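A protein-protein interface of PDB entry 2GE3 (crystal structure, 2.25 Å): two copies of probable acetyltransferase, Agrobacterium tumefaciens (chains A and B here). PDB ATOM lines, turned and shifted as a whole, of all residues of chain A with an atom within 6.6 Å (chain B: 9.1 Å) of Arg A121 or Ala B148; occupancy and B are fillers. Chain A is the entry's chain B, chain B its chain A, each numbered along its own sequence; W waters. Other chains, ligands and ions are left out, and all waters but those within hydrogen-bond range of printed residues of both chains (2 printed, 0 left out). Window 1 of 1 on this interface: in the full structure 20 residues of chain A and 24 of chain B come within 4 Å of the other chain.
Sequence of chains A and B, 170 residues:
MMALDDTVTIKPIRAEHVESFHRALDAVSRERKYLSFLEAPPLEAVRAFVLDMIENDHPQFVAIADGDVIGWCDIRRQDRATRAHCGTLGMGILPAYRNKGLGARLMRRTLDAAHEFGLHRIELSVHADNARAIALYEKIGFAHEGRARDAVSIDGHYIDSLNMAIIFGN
SG of Cys A86 lies within hydrogen-bond range of O of Ala B151, at 3.4 Å. The side-chain carboxylate of Glu A145 sits at hydrogen-bond distance from the backbone NH of Arg B149 (3.2 Å). The guanidinium group (NH1) of Arg A121 lies within hydrogen-bond range of the backbone carbonyl oxygen (O) of Arg B149 (2.8 Å). The backbone carbonyl oxygen (O) of Ala B151 sits at hydrogen-bond distance from the guanidinium group (NH1) of Arg A83, 2.8 Å away. NE2 of His A120 is in hydrogen-bond range of OD2 of Asp B150 (2.8 Å). O of Glu A145 lies within hydrogen-bond range of N of Arg B147 (3.3 Å). O of Asp B150 sits at hydrogen-bond distance from NE2 of His A85, 2.7 Å away.
N of Ala B151 lies within hydrogen-bond range of O of Ile B159, 3.1 Å away. NH1 of Arg A83 is in hydrogen-bond range of SG of Cys A86 (3.3 Å). The side-chain sulfur of Cys A86 sits close to a ring nitrogen (NE2) of His A85. OD1 of Asp B160 lies within hydrogen-bond range of N of Asp B150 (3.0 Å). O of Ser B161 is in hydrogen-bond range of N of Ala B148. The backbone NH (N) of Phe A168 lies within hydrogen-bond range of the backbone carbonyl oxygen (O) of His A120, 2.8 Å away.
Among the printed residues, pairs that only touch across the chains: Glu A145 with Gly B146, His A85 with Ala B151, His A85 with Tyr B158, Glu A145 with Ala B148, Arg A121 with Ala B148, His A120 with Tyr B158, Arg A121 with Asp B150, His A85 with Ser B153, Ile A167 with Arg B149, His A85 with Val B152 and Arg A121 with Ala B151.
Arg A121 touches just these residues of chain B: Ala B148 (3.5 Å), Arg B149 (2.8 Å), Asp B150 (3.6 Å) and Ala B151 (3.8 Å). Of the printed residues of chain B, Cys A86 touches Ala B151. Printed residues of chain A within 4 Å of Ala B151: Arg A83 (2.8 Å), His A85 (3.2 Å), Cys A86 (3.4 Å) and Arg A121 (3.8 Å). Printed residues of chain A within 4 Å of Val B152: His A85 (3.7 Å). Printed residues of chain A within 4 Å of Asp B150: His A85 (2.7 Å), His A120 (2.8 Å) and Arg A121 (3.6 Å). Glu B145 touches none of the printed residues of chain A. The nearest residue of chain A that does not touch Ala B148 is Glu A123 (5.4 Å).
Positions printed for both chains: 145 and 164. Of the 18 pairs that touch across the chains among the printed residues, none has its exchanged pair printed and touching as well.
Of the 20 printed residues of chain B, 9 touch a printed residue of chain A. Printed residues of chain B that touch a printed residue of chain A: Gly B146, Arg B147, Ala B148, Arg B149, Asp B150, Ala B151, Val B152, Ser B153 and Tyr B158. Hydrophobic or aromatic side chains of chain B within 4 Å of the printed part of chain A: Ala B148, Ala B151 and Tyr B158. Hydrophobic or aromatic side chains of chain A within 4 Å of the printed part of chain B: His A85, His A120 and Ile A167. Among the printed residues, 18 pairs touch across the chains. Among the printed residues, no Asp or Glu carboxylate lies within 4 Å of a Lys or Arg side-chain nitrogen of the other chain.
Water W2 bridges ND2 of Asn B163 (2.6 Å) and O of Glu A145 (3.2 Å). Water W1 bridges N of Arg B147 (3.3 Å) and O of Glu A145 (3.5 Å).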
ATOM      1  N   ILE A  75       2.136 -17.249  26.159  1.00  0.00           N
ATOM      2  CA  ILE A  75       1.104 -17.389  25.139  1.00  0.00           C
ATOM      3  C   ILE A  75       0.218 -18.529  25.535  1.00  0.00           C
ATOM      4  O   ILE A  75       0.689 -19.614  25.671  1.00  0.00           O
ATOM      5  CB  ILE A  75       1.736 -17.601  23.705  1.00  0.00           C
ATOM      6  CG1 ILE A  75       2.378 -16.285  23.250  1.00  0.00           C
ATOM      7  CG2 ILE A  75       0.622 -18.024  22.661  1.00  0.00           C
ATOM      8  CD1 ILE A  75       3.469 -16.411  22.079  1.00  0.00           C
ATOM      9  N   ARG A  83     -10.598 -21.831  17.178  1.00  0.00           N
ATOM     10  CA  ARG A  83      -9.657 -20.862  17.648  1.00  0.00           C
ATOM     11  C   ARG A  83      -8.298 -21.435  18.088  1.00  0.00           C
ATOM     12  O   ARG A  83      -7.387 -20.681  18.357  1.00  0.00           O
ATOM     13  CB  ARG A  83     -10.334 -20.031  18.751  1.00  0.00           C
ATOM     14  CG  ARG A  83     -11.645 -19.389  18.253  1.00  0.00           C
ATOM     15  CD  ARG A  83     -11.536 -17.962  17.633  1.00  0.00           C
ATOM     16  NE  ARG A  83     -11.020 -17.095  18.682  1.00  0.00           N
ATOM     17  CZ  ARG A  83      -9.936 -16.310  18.593  1.00  0.00           C
ATOM     18  NH1 ARG A  83      -9.251 -16.224  17.469  1.00  0.00           N
ATOM     19  NH2 ARG A  83      -9.544 -15.599  19.657  1.00  0.00           N
ATOM     20  N   HIS A  85      -5.717 -22.596  16.595  1.00  0.00           N
ATOM     21  CA  HIS A  85      -4.518 -22.069  15.872  1.00  0.00           C
ATOM     22  C   HIS A  85      -4.033 -20.675  16.419  1.00  0.00           C
ATOM     23  O   HIS A  85      -3.073 -20.123  15.881  1.00  0.00           O
ATOM     24  CB  HIS A  85      -4.814 -21.968  14.405  1.00  0.00           C
ATOM     25  CG  HIS A  85      -5.826 -20.901  14.064  1.00  0.00           C
ATOM     26  ND1 HIS A  85      -7.123 -20.901  14.562  1.00  0.00           N
ATOM     27  CD2 HIS A  85      -5.725 -19.794  13.291  1.00  0.00           C
ATOM     28  CE1 HIS A  85      -7.773 -19.841  14.104  1.00  0.00           C
ATOM     29  NE2 HIS A  85      -6.944 -19.162  13.327  1.00  0.00           N
ATOM     30  N   CYS A  86      -4.723 -20.119  17.449  1.00  0.00           N
ATOM     31  CA  CYS A  86      -4.384 -18.802  17.984  1.00  0.00           C
ATOM     32  C   CYS A  86      -3.978 -18.896  19.410  1.00  0.00           C
ATOM     33  O   CYS A  86      -4.457 -19.764  20.110  1.00  0.00           O
ATOM     34  CB  CYS A  86      -5.562 -17.771  17.911  1.00  0.00           C
ATOM     35  SG  CYS A  86      -6.579 -17.754  16.392  1.00  0.00           S
ATOM     36  N   GLY A  87      -3.120 -17.975  19.844  1.00  0.00           N
ATOM     37  CA  GLY A  87      -2.774 -17.807  21.233  1.00  0.00           C
ATOM     38  C   GLY A  87      -2.838 -16.323  21.693  1.00  0.00           C
ATOM     39  O   GLY A  87      -2.875 -15.420  20.879  1.00  0.00           O
ATOM     40  N   THR A  88      -2.969 -16.104  22.997  1.00  0.00           N
ATOM     41  CA  THR A  88      -3.070 -14.784  23.596  1.00  0.00           C
ATOM     42  C   THR A  88      -1.833 -14.524  24.396  1.00  0.00           C
ATOM     43  O   THR A  88      -1.474 -15.279  25.262  1.00  0.00           O
ATOM     44  CB  THR A  88      -4.256 -14.634  24.492  1.00  0.00           C
ATOM     45  OG1 THR A  88      -5.438 -14.881  23.706  1.00  0.00           O
ATOM     46  CG2 THR A  88      -4.332 -13.162  25.082  1.00  0.00           C
ATOM     47  N   GLY A 118       3.421 -24.599  16.639  1.00  0.00           N
ATOM     48  CA  GLY A 118       2.568 -24.695  15.478  1.00  0.00           C
ATOM     49  C   GLY A 118       1.395 -23.724  15.484  1.00  0.00           C
ATOM     50  O   GLY A 118       0.475 -23.869  14.696  1.00  0.00           O
ATOM     51  N   LEU A 119       1.399 -22.714  16.344  1.00  0.00           N
ATOM     52  CA  LEU A 119       0.338 -21.682  16.257  1.00  0.00           C
ATOM     53  C   LEU A 119       0.517 -20.839  14.992  1.00  0.00           C
ATOM     54  O   LEU A 119       1.588 -20.656  14.529  1.00  0.00           O
ATOM     55  CB  LEU A 119       0.363 -20.781  17.494  1.00  0.00           C
ATOM     56  CG  LEU A 119       0.144 -21.611  18.774  1.00  0.00           C
ATOM     57  CD1 LEU A 119       0.124 -20.675  20.007  1.00  0.00           C
ATOM     58  CD2 LEU A 119      -1.234 -22.310  18.658  1.00  0.00           C
ATOM     59  N   HIS A 120      -0.571 -20.331  14.466  1.00  0.00           N
ATOM     60  CA  HIS A 120      -0.600 -19.455  13.300  1.00  0.00           C
ATOM     61  C   HIS A 120      -0.705 -17.971  13.688  1.00  0.00           C
ATOM     62  O   HIS A 120      -0.169 -17.110  12.996  1.00  0.00           O
ATOM     63  CB  HIS A 120      -1.823 -19.872  12.434  1.00  0.00           C
ATOM     64  CG  HIS A 120      -2.060 -19.024  11.248  1.00  0.00           C
ATOM     65  ND1 HIS A 120      -1.218 -19.029  10.162  1.00  0.00           N
ATOM     66  CD2 HIS A 120      -3.080 -18.178  10.935  1.00  0.00           C
ATOM     67  CE1 HIS A 120      -1.683 -18.210   9.232  1.00  0.00           C
ATOM     68  NE2 HIS A 120      -2.828 -17.691   9.671  1.00  0.00           N
ATOM     69  N   ARG A 121      -1.352 -17.676  14.827  1.00  0.00           N
ATOM     70  CA  ARG A 121      -1.758 -16.338  15.097  1.00  0.00           C
ATOM     71  C   ARG A 121      -1.610 -16.030  16.562  1.00  0.00           C
ATOM     72  O   ARG A 121      -2.091 -16.802  17.433  1.00  0.00           O
ATOM     73  CB  ARG A 121      -3.198 -16.149  14.591  1.00  0.00           C
ATOM     74  CG  ARG A 121      -3.887 -14.837  15.081  1.00  0.00           C
ATOM     75  CD  ARG A 121      -5.304 -14.712  14.487  1.00  0.00           C
ATOM     76  NE  ARG A 121      -5.928 -13.647  15.245  1.00  0.00           N
ATOM     77  CZ  ARG A 121      -5.910 -12.356  14.900  1.00  0.00           C
ATOM     78  NH1 ARG A 121      -5.424 -11.953  13.732  1.00  0.00           N
ATOM     79  NH2 ARG A 121      -6.466 -11.473  15.716  1.00  0.00           N
ATOM     80  N   ILE A 122      -0.854 -14.962  16.874  1.00  0.00           N
ATOM     81  CA  ILE A 122      -0.743 -14.533  18.239  1.00  0.00           C
ATOM     82  C   ILE A 122      -1.476 -13.152  18.404  1.00  0.00           C
ATOM     83  O   ILE A 122      -1.206 -12.228  17.679  1.00  0.00           O
ATOM     84  CB  ILE A 122       0.714 -14.333  18.663  1.00  0.00           C
ATOM     85  CG1 ILE A 122       1.561 -15.559  18.308  1.00  0.00           C
ATOM     86  CG2 ILE A 122       0.775 -13.919  20.144  1.00  0.00           C
ATOM     87  CD1 ILE A 122       0.964 -16.950  18.780  1.00  0.00           C
ATOM     88  N   GLU A 123      -2.340 -13.036  19.387  1.00  0.00           N
ATOM     89  CA  GLU A 123      -3.057 -11.793  19.606  1.00  0.00           C
ATOM     90  C   GLU A 123      -2.801 -11.242  21.001  1.00  0.00           C
ATOM     91  O   GLU A 123      -2.423 -11.963  21.921  1.00  0.00           O
ATOM     92  CB  GLU A 123      -4.541 -11.900  19.239  1.00  0.00           C
ATOM     93  CG  GLU A 123      -5.301 -12.738  20.088  1.00  0.00           C
ATOM     94  CD  GLU A 123      -6.634 -13.396  19.375  1.00  0.00           C
ATOM     95  OE1 GLU A 123      -7.469 -13.825  20.188  1.00  0.00           O
ATOM     96  OE2 GLU A 123      -6.877 -13.521  18.103  1.00  0.00           O
ATOM     97  N   GLU A 145      -5.140  -3.985  14.954  1.00  0.00           N
ATOM     98  CA  GLU A 145      -6.366  -4.551  14.364  1.00  0.00           C
ATOM     99  C   GLU A 145      -7.624  -3.813  14.882  1.00  0.00           C
ATOM    100  O   GLU A 145      -8.699  -4.178  14.517  1.00  0.00           O
ATOM    101  CB  GLU A 145      -6.512  -6.040  14.738  1.00  0.00           C
ATOM    102  CG  GLU A 145      -5.472  -6.880  14.043  1.00  0.00           C
ATOM    103  CD  GLU A 145      -5.813  -8.381  13.963  1.00  0.00           C
ATOM    104  OE1 GLU A 145      -5.462  -8.981  12.915  1.00  0.00           O
ATOM    105  OE2 GLU A 145      -6.392  -8.927  14.971  1.00  0.00           O
ATOM    106  N   MET A 164      -4.119  -6.173  18.830  1.00  0.00           N
ATOM    107  CA  MET A 164      -2.980  -6.216  17.919  1.00  0.00           C
ATOM    108  C   MET A 164      -2.732  -7.664  17.635  1.00  0.00           C
ATOM    109  O   MET A 164      -3.116  -8.497  18.430  1.00  0.00           O
ATOM    110  CB  MET A 164      -1.746  -5.632  18.592  1.00  0.00           C
ATOM    111  CG  MET A 164      -1.970  -4.138  18.974  1.00  0.00           C
ATOM    112  SD  MET A 164      -0.202  -3.296  19.470  1.00  0.00           S
ATOM    113  CE  MET A 164       0.792  -3.149  17.629  1.00  0.00           C
ATOM    114  N   ALA A 165      -2.049  -7.989  16.532  1.00  0.00           N
ATOM    115  CA  ALA A 165      -1.883  -9.379  16.232  1.00  0.00           C
ATOM    116  C   ALA A 165      -0.747  -9.606  15.353  1.00  0.00           C
ATOM    117  O   ALA A 165      -0.293  -8.732  14.704  1.00  0.00           O
ATOM    118  CB  ALA A 165      -3.156  -9.943  15.596  1.00  0.00           C
ATOM    119  N   ILE A 166      -0.211 -10.790  15.400  1.00  0.00           N
ATOM    120  CA  ILE A 166       0.866 -11.115  14.528  1.00  0.00           C
ATOM    121  C   ILE A 166       0.535 -12.501  13.984  1.00  0.00           C
ATOM    122  O   ILE A 166      -0.156 -13.319  14.653  1.00  0.00           O
ATOM    123  CB  ILE A 166       2.223 -11.035  15.247  1.00  0.00           C
ATOM    124  CG1 ILE A 166       3.340 -10.786  14.221  1.00  0.00           C
ATOM    125  CG2 ILE A 166       2.500 -12.326  15.985  1.00  0.00           C
ATOM    126  CD1 ILE A 166       4.778 -10.582  14.903  1.00  0.00           C
ATOM    127  N   ILE A 167       0.938 -12.750  12.764  1.00  0.00           N
ATOM    128  CA  ILE A 167       0.558 -14.001  12.021  1.00  0.00           C
ATOM    129  C   ILE A 167       1.823 -14.591  11.499  1.00  0.00           C
ATOM    130  O   ILE A 167       2.589 -13.905  10.831  1.00  0.00           O
ATOM    131  CB  ILE A 167      -0.370 -13.710  10.836  1.00  0.00           C
ATOM    132  CG1 ILE A 167      -1.733 -13.402  11.355  1.00  0.00           C
ATOM    133  CG2 ILE A 167      -0.428 -14.910   9.836  1.00  0.00           C
ATOM    134  CD1 ILE A 167      -2.646 -13.200  10.313  1.00  0.00           C
ATOM    135  N   PHE A 168       2.098 -15.832  11.860  1.00  0.00           N
ATOM    136  CA  PHE A 168       3.375 -16.415  11.420  1.00  0.00           C
ATOM    137  C   PHE A 168       3.445 -16.735   9.936  1.00  0.00           C
ATOM    138  O   PHE A 168       2.526 -17.318   9.342  1.00  0.00           O
ATOM    139  CB  PHE A 168       3.798 -17.636  12.235  1.00  0.00           C
ATOM    140  CG  PHE A 168       4.066 -17.339  13.634  1.00  0.00           C
ATOM    141  CD1 PHE A 168       3.349 -17.990  14.627  1.00  0.00           C
ATOM    142  CD2 PHE A 168       5.058 -16.416  13.980  1.00  0.00           C
ATOM    143  CE1 PHE A 168       3.594 -17.691  15.960  1.00  0.00           C
ATOM    144  CE2 PHE A 168       5.282 -16.122  15.295  1.00  0.00           C
ATOM    145  CZ  PHE A 168       4.533 -16.765  16.294  1.00  0.00           C
ATOM    146  N   SER B 125     -18.104 -10.933  18.499  1.00  0.00           N
ATOM    147  CA  SER B 125     -17.249 -11.271  17.359  1.00  0.00           C
ATOM    148  C   SER B 125     -18.100 -11.953  16.307  1.00  0.00           C
ATOM    149  O   SER B 125     -18.893 -12.784  16.669  1.00  0.00           O
ATOM    150  CB  SER B 125     -16.197 -12.250  17.834  1.00  0.00           C
ATOM    151  OG  SER B 125     -15.183 -11.408  18.436  1.00  0.00           O
ATOM    152  N   VAL B 126     -17.942 -11.615  15.034  1.00  0.00           N
ATOM    153  CA  VAL B 126     -18.711 -12.208  13.969  1.00  0.00           C
ATOM    154  C   VAL B 126     -17.808 -12.574  12.769  1.00  0.00           C
ATOM    155  O   VAL B 126     -16.890 -11.812  12.433  1.00  0.00           O
ATOM    156  CB  VAL B 126     -19.904 -11.255  13.575  1.00  0.00           C
ATOM    157  CG1 VAL B 126     -19.380  -9.859  13.039  1.00  0.00           C
ATOM    158  CG2 VAL B 126     -20.809 -11.875  12.631  1.00  0.00           C
ATOM    159  N   HIS B 127     -18.080 -13.715  12.123  1.00  0.00           N
ATOM    160  CA  HIS B 127     -17.349 -14.078  10.929  1.00  0.00           C
ATOM    161  C   HIS B 127     -17.550 -13.056   9.844  1.00  0.00           C
ATOM    162  O   HIS B 127     -18.686 -12.611   9.583  1.00  0.00           O
ATOM    163  CB  HIS B 127     -17.688 -15.510  10.423  1.00  0.00           C
ATOM    164  CG  HIS B 127     -17.433 -16.606  11.410  1.00  0.00           C
ATOM    165  ND1 HIS B 127     -17.859 -17.898  11.212  1.00  0.00           N
ATOM    166  CD2 HIS B 127     -16.804 -16.615  12.613  1.00  0.00           C
ATOM    167  CE1 HIS B 127     -17.552 -18.639  12.261  1.00  0.00           C
ATOM    168  NE2 HIS B 127     -16.945 -17.875  13.142  1.00  0.00           N
ATOM    169  N   ALA B 128     -16.453 -12.690   9.170  1.00  0.00           N
ATOM    170  CA  ALA B 128     -16.482 -11.585   8.185  1.00  0.00           C
ATOM    171  C   ALA B 128     -17.420 -11.892   7.019  1.00  0.00           C
ATOM    172  O   ALA B 128     -17.929 -10.975   6.332  1.00  0.00           O
ATOM    173  CB  ALA B 128     -15.078 -11.166   7.665  1.00  0.00           C
ATOM    174  N   GLU B 145     -15.329  -2.337  15.359  1.00  0.00           N
ATOM    175  CA  GLU B 145     -14.188  -1.994  16.200  1.00  0.00           C
ATOM    176  C   GLU B 145     -12.902  -2.541  15.677  1.00  0.00           C
ATOM    177  O   GLU B 145     -11.901  -2.170  16.223  1.00  0.00           O
ATOM    178  CB  GLU B 145     -14.330  -2.496  17.637  1.00  0.00           C
ATOM    179  CG  GLU B 145     -15.340  -1.653  18.400  1.00  0.00           C
ATOM    180  CD  GLU B 145     -15.196  -1.837  19.912  1.00  0.00           C
ATOM    181  OE1 GLU B 145     -15.403  -0.845  20.649  1.00  0.00           O
ATOM    182  OE2 GLU B 145     -14.870  -2.997  20.344  1.00  0.00           O
ATOM    183  N   GLY B 146     -12.960  -3.407  14.660  1.00  0.00           N
ATOM    184  CA  GLY B 146     -11.822  -3.872  13.951  1.00  0.00           C
ATOM    185  C   GLY B 146     -11.949  -5.276  13.416  1.00  0.00           C
ATOM    186  O   GLY B 146     -12.925  -5.936  13.691  1.00  0.00           O
ATOM    187  N   ARG B 147     -10.927  -5.756  12.677  1.00  0.00           N
ATOM    188  CA  ARG B 147     -11.046  -6.972  11.861  1.00  0.00           C
ATOM    189  C   ARG B 147      -9.905  -7.851  12.351  1.00  0.00           C
ATOM    190  O   ARG B 147      -8.779  -7.415  12.435  1.00  0.00           O
ATOM    191  CB  ARG B 147     -10.873  -6.551  10.421  1.00  0.00           C
ATOM    192  CG  ARG B 147     -10.699  -7.614   9.440  1.00  0.00           C
ATOM    193  CD  ARG B 147     -10.771  -6.978   8.078  1.00  0.00           C
ATOM    194  NE  ARG B 147     -11.643  -7.701   7.155  1.00  0.00           N
ATOM    195  CZ  ARG B 147     -12.790  -7.188   6.682  1.00  0.00           C
ATOM    196  NH1 ARG B 147     -13.173  -5.952   6.993  1.00  0.00           N
ATOM    197  NH2 ARG B 147     -13.555  -7.898   5.892  1.00  0.00           N
ATOM    198  N   ALA B 148     -10.204  -9.072  12.756  1.00  0.00           N
ATOM    199  CA  ALA B 148      -9.155  -9.998  13.152  1.00  0.00           C
ATOM    200  C   ALA B 148      -8.784 -10.958  12.000  1.00  0.00           C
ATOM    201  O   ALA B 148      -9.568 -11.764  11.689  1.00  0.00           O
ATOM    202  CB  ALA B 148      -9.639 -10.764  14.422  1.00  0.00           C
ATOM    203  N   ARG B 149      -7.567 -10.903  11.430  1.00  0.00           N
ATOM    204  CA  ARG B 149      -7.246 -11.675  10.236  1.00  0.00           C
ATOM    205  C   ARG B 149      -6.975 -13.135  10.583  1.00  0.00           C
ATOM    206  O   ARG B 149      -6.171 -13.394  11.446  1.00  0.00           O
ATOM    207  CB  ARG B 149      -5.987 -11.127   9.494  1.00  0.00           C
ATOM    208  CG  ARG B 149      -5.951  -9.576   9.405  1.00  0.00           C
ATOM    209  CD  ARG B 149      -6.860  -8.982   8.244  1.00  0.00           C
ATOM    210  NE  ARG B 149      -6.903  -9.784   6.990  1.00  0.00           N
ATOM    211  CZ  ARG B 149      -5.977  -9.800   6.002  1.00  0.00           C
ATOM    212  NH1 ARG B 149      -4.876  -9.039   6.009  1.00  0.00           N
ATOM    213  NH2 ARG B 149      -6.178 -10.577   4.939  1.00  0.00           N
ATOM    214  N   ASP B 150      -7.571 -14.058   9.835  1.00  0.00           N
ATOM    215  CA  ASP B 150      -7.356 -15.484  10.112  1.00  0.00           C
ATOM    216  C   ASP B 150      -7.672 -15.901  11.578  1.00  0.00           C
ATOM    217  O   ASP B 150      -7.017 -16.733  12.119  1.00  0.00           O
ATOM    218  CB  ASP B 150      -5.910 -15.910   9.811  1.00  0.00           C
ATOM    219  CG  ASP B 150      -5.536 -15.812   8.325  1.00  0.00           C
ATOM    220  OD1 ASP B 150      -6.483 -15.529   7.508  1.00  0.00           O
ATOM    221  OD2 ASP B 150      -4.272 -16.032   8.002  1.00  0.00           O
ATOM    222  N   ALA B 151      -8.651 -15.321  12.195  1.00  0.00           N
ATOM    223  CA  ALA B 151      -8.884 -15.560  13.629  1.00  0.00           C
ATOM    224  C   ALA B 151      -9.681 -16.864  13.853  1.00  0.00           C
ATOM    225  O   ALA B 151      -9.667 -17.386  14.945  1.00  0.00           O
ATOM    226  CB  ALA B 151      -9.586 -14.382  14.289  1.00  0.00           C
ATOM    227  N   VAL B 152     -10.287 -17.400  12.789  1.00  0.00           N
ATOM    228  CA  VAL B 152     -11.253 -18.539  12.848  1.00  0.00           C
ATOM    229  C   VAL B 152     -10.715 -19.566  11.851  1.00  0.00           C
ATOM    230  O   VAL B 152     -10.209 -19.214  10.796  1.00  0.00           O
ATOM    231  CB  VAL B 152     -12.737 -18.064  12.539  1.00  0.00           C
ATOM    232  CG1 VAL B 152     -13.740 -19.253  12.369  1.00  0.00           C
ATOM    233  CG2 VAL B 152     -13.284 -17.202  13.638  1.00  0.00           C
ATOM    234  N   SER B 153     -10.725 -20.827  12.197  1.00  0.00           N
ATOM    235  CA  SER B 153     -10.350 -21.866  11.207  1.00  0.00           C
ATOM    236  C   SER B 153     -11.466 -22.895  11.343  1.00  0.00           C
ATOM    237  O   SER B 153     -11.829 -23.252  12.475  1.00  0.00           O
ATOM    238  CB  SER B 153      -9.023 -22.498  11.602  1.00  0.00           C
ATOM    239  OG  SER B 153      -8.590 -23.465  10.692  1.00  0.00           O
ATOM    240  N   TYR B 158      -9.059 -20.663   6.902  1.00  0.00           N
ATOM    241  CA  TYR B 158      -9.049 -19.428   7.721  1.00  0.00           C
ATOM    242  C   TYR B 158     -10.116 -18.417   7.345  1.00  0.00           C
ATOM    243  O   TYR B 158     -10.227 -18.042   6.187  1.00  0.00           O
ATOM    244  CB  TYR B 158      -7.687 -18.716   7.645  1.00  0.00           C
ATOM    245  CG  TYR B 158      -6.552 -19.517   8.225  1.00  0.00           C
ATOM    246  CD1 TYR B 158      -5.425 -19.800   7.470  1.00  0.00           C
ATOM    247  CD2 TYR B 158      -6.621 -20.032   9.526  1.00  0.00           C
ATOM    248  CE1 TYR B 158      -4.401 -20.606   7.981  1.00  0.00           C
ATOM    249  CE2 TYR B 158      -5.561 -20.802  10.061  1.00  0.00           C
ATOM    250  CZ  TYR B 158      -4.479 -21.087   9.297  1.00  0.00           C
ATOM    251  OH  TYR B 158      -3.472 -21.896   9.822  1.00  0.00           O
ATOM    252  N   ILE B 159     -10.827 -17.933   8.360  1.00  0.00           N
ATOM    253  CA  ILE B 159     -11.875 -16.888   8.274  1.00  0.00           C
ATOM    254  C   ILE B 159     -11.445 -15.683   9.139  1.00  0.00           C
ATOM    255  O   ILE B 159     -10.984 -15.834  10.268  1.00  0.00           O
ATOM    256  CB  ILE B 159     -13.294 -17.404   8.843  1.00  0.00           C
ATOM    257  CG1 ILE B 159     -13.625 -18.826   8.398  1.00  0.00           C
ATOM    258  CG2 ILE B 159     -14.456 -16.514   8.465  1.00  0.00           C
ATOM    259  CD1 ILE B 159     -13.427 -19.019   6.977  1.00  0.00           C
ATOM    260  N   ASP B 160     -11.605 -14.492   8.598  1.00  0.00           N
ATOM    261  CA  ASP B 160     -11.572 -13.281   9.406  1.00  0.00           C
ATOM    262  C   ASP B 160     -12.762 -13.144  10.331  1.00  0.00           C
ATOM    263  O   ASP B 160     -13.898 -13.595  10.081  1.00  0.00           O
ATOM    264  CB  ASP B 160     -11.495 -12.077   8.470  1.00  0.00           C
ATOM    265  CG  ASP B 160     -10.153 -12.026   7.697  1.00  0.00           C
ATOM    266  OD1 ASP B 160      -9.379 -12.989   7.746  1.00  0.00           O
ATOM    267  OD2 ASP B 160      -9.863 -11.025   7.033  1.00  0.00           O
ATOM    268  N   SER B 161     -12.497 -12.488  11.423  1.00  0.00           N
ATOM    269  CA  SER B 161     -13.574 -12.211  12.368  1.00  0.00           C
ATOM    270  C   SER B 161     -13.643 -10.673  12.511  1.00  0.00           C
ATOM    271  O   SER B 161     -12.639 -10.007  12.436  1.00  0.00           O
ATOM    272  CB  SER B 161     -13.243 -12.850  13.731  1.00  0.00           C
ATOM    273  OG  SER B 161     -14.453 -13.142  14.367  1.00  0.00           O
ATOM    274  N   LEU B 162     -14.823 -10.129  12.684  1.00  0.00           N
ATOM    275  CA  LEU B 162     -15.010  -8.695  12.935  1.00  0.00           C
ATOM    276  C   LEU B 162     -15.424  -8.524  14.329  1.00  0.00           C
ATOM    277  O   LEU B 162     -16.354  -9.207  14.817  1.00  0.00           O
ATOM    278  CB  LEU B 162     -16.125  -8.106  12.063  1.00  0.00           C
ATOM    279  CG  LEU B 162     -15.950  -8.303  10.539  1.00  0.00           C
ATOM    280  CD1 LEU B 162     -17.055  -7.618   9.713  1.00  0.00           C
ATOM    281  CD2 LEU B 162     -14.543  -7.915  10.003  1.00  0.00           C
ATOM    282  N   ASN B 163     -14.786  -7.574  14.976  1.00  0.00           N
ATOM    283  CA  ASN B 163     -15.194  -7.213  16.358  1.00  0.00           C
ATOM    284  C   ASN B 163     -16.079  -6.036  16.338  1.00  0.00           C
ATOM    285  O   ASN B 163     -15.789  -5.089  15.653  1.00  0.00           O
ATOM    286  CB  ASN B 163     -13.970  -6.843  17.208  1.00  0.00           C
ATOM    287  CG  ASN B 163     -13.111  -8.036  17.429  1.00  0.00           C
ATOM    288  OD1 ASN B 163     -13.625  -8.994  17.907  1.00  0.00           O
ATOM    289  ND2 ASN B 163     -11.852  -8.031  16.962  1.00  0.00           N
ATOM    290  N   MET B 164     -17.115  -6.062  17.138  1.00  0.00           N
ATOM    291  CA  MET B 164     -18.099  -4.990  17.107  1.00  0.00           C
ATOM    292  C   MET B 164     -18.494  -4.795  18.558  1.00  0.00           C
ATOM    293  O   MET B 164     -18.343  -5.709  19.342  1.00  0.00           O
ATOM    294  CB  MET B 164     -19.299  -5.390  16.257  1.00  0.00           C
ATOM    295  CG  MET B 164     -18.894  -5.785  14.739  1.00  0.00           C
ATOM    296  SD  MET B 164     -20.643  -6.041  13.833  1.00  0.00           S
ATOM    297  CE  MET B 164     -21.167  -4.062  13.683  1.00  0.00           C
HETATM  298  O   HOH W   1      -8.999  -3.630  11.116  1.00  0.00           O
HETATM  299  O   HOH W   2     -10.054  -6.227  16.529  1.00  0.00           O
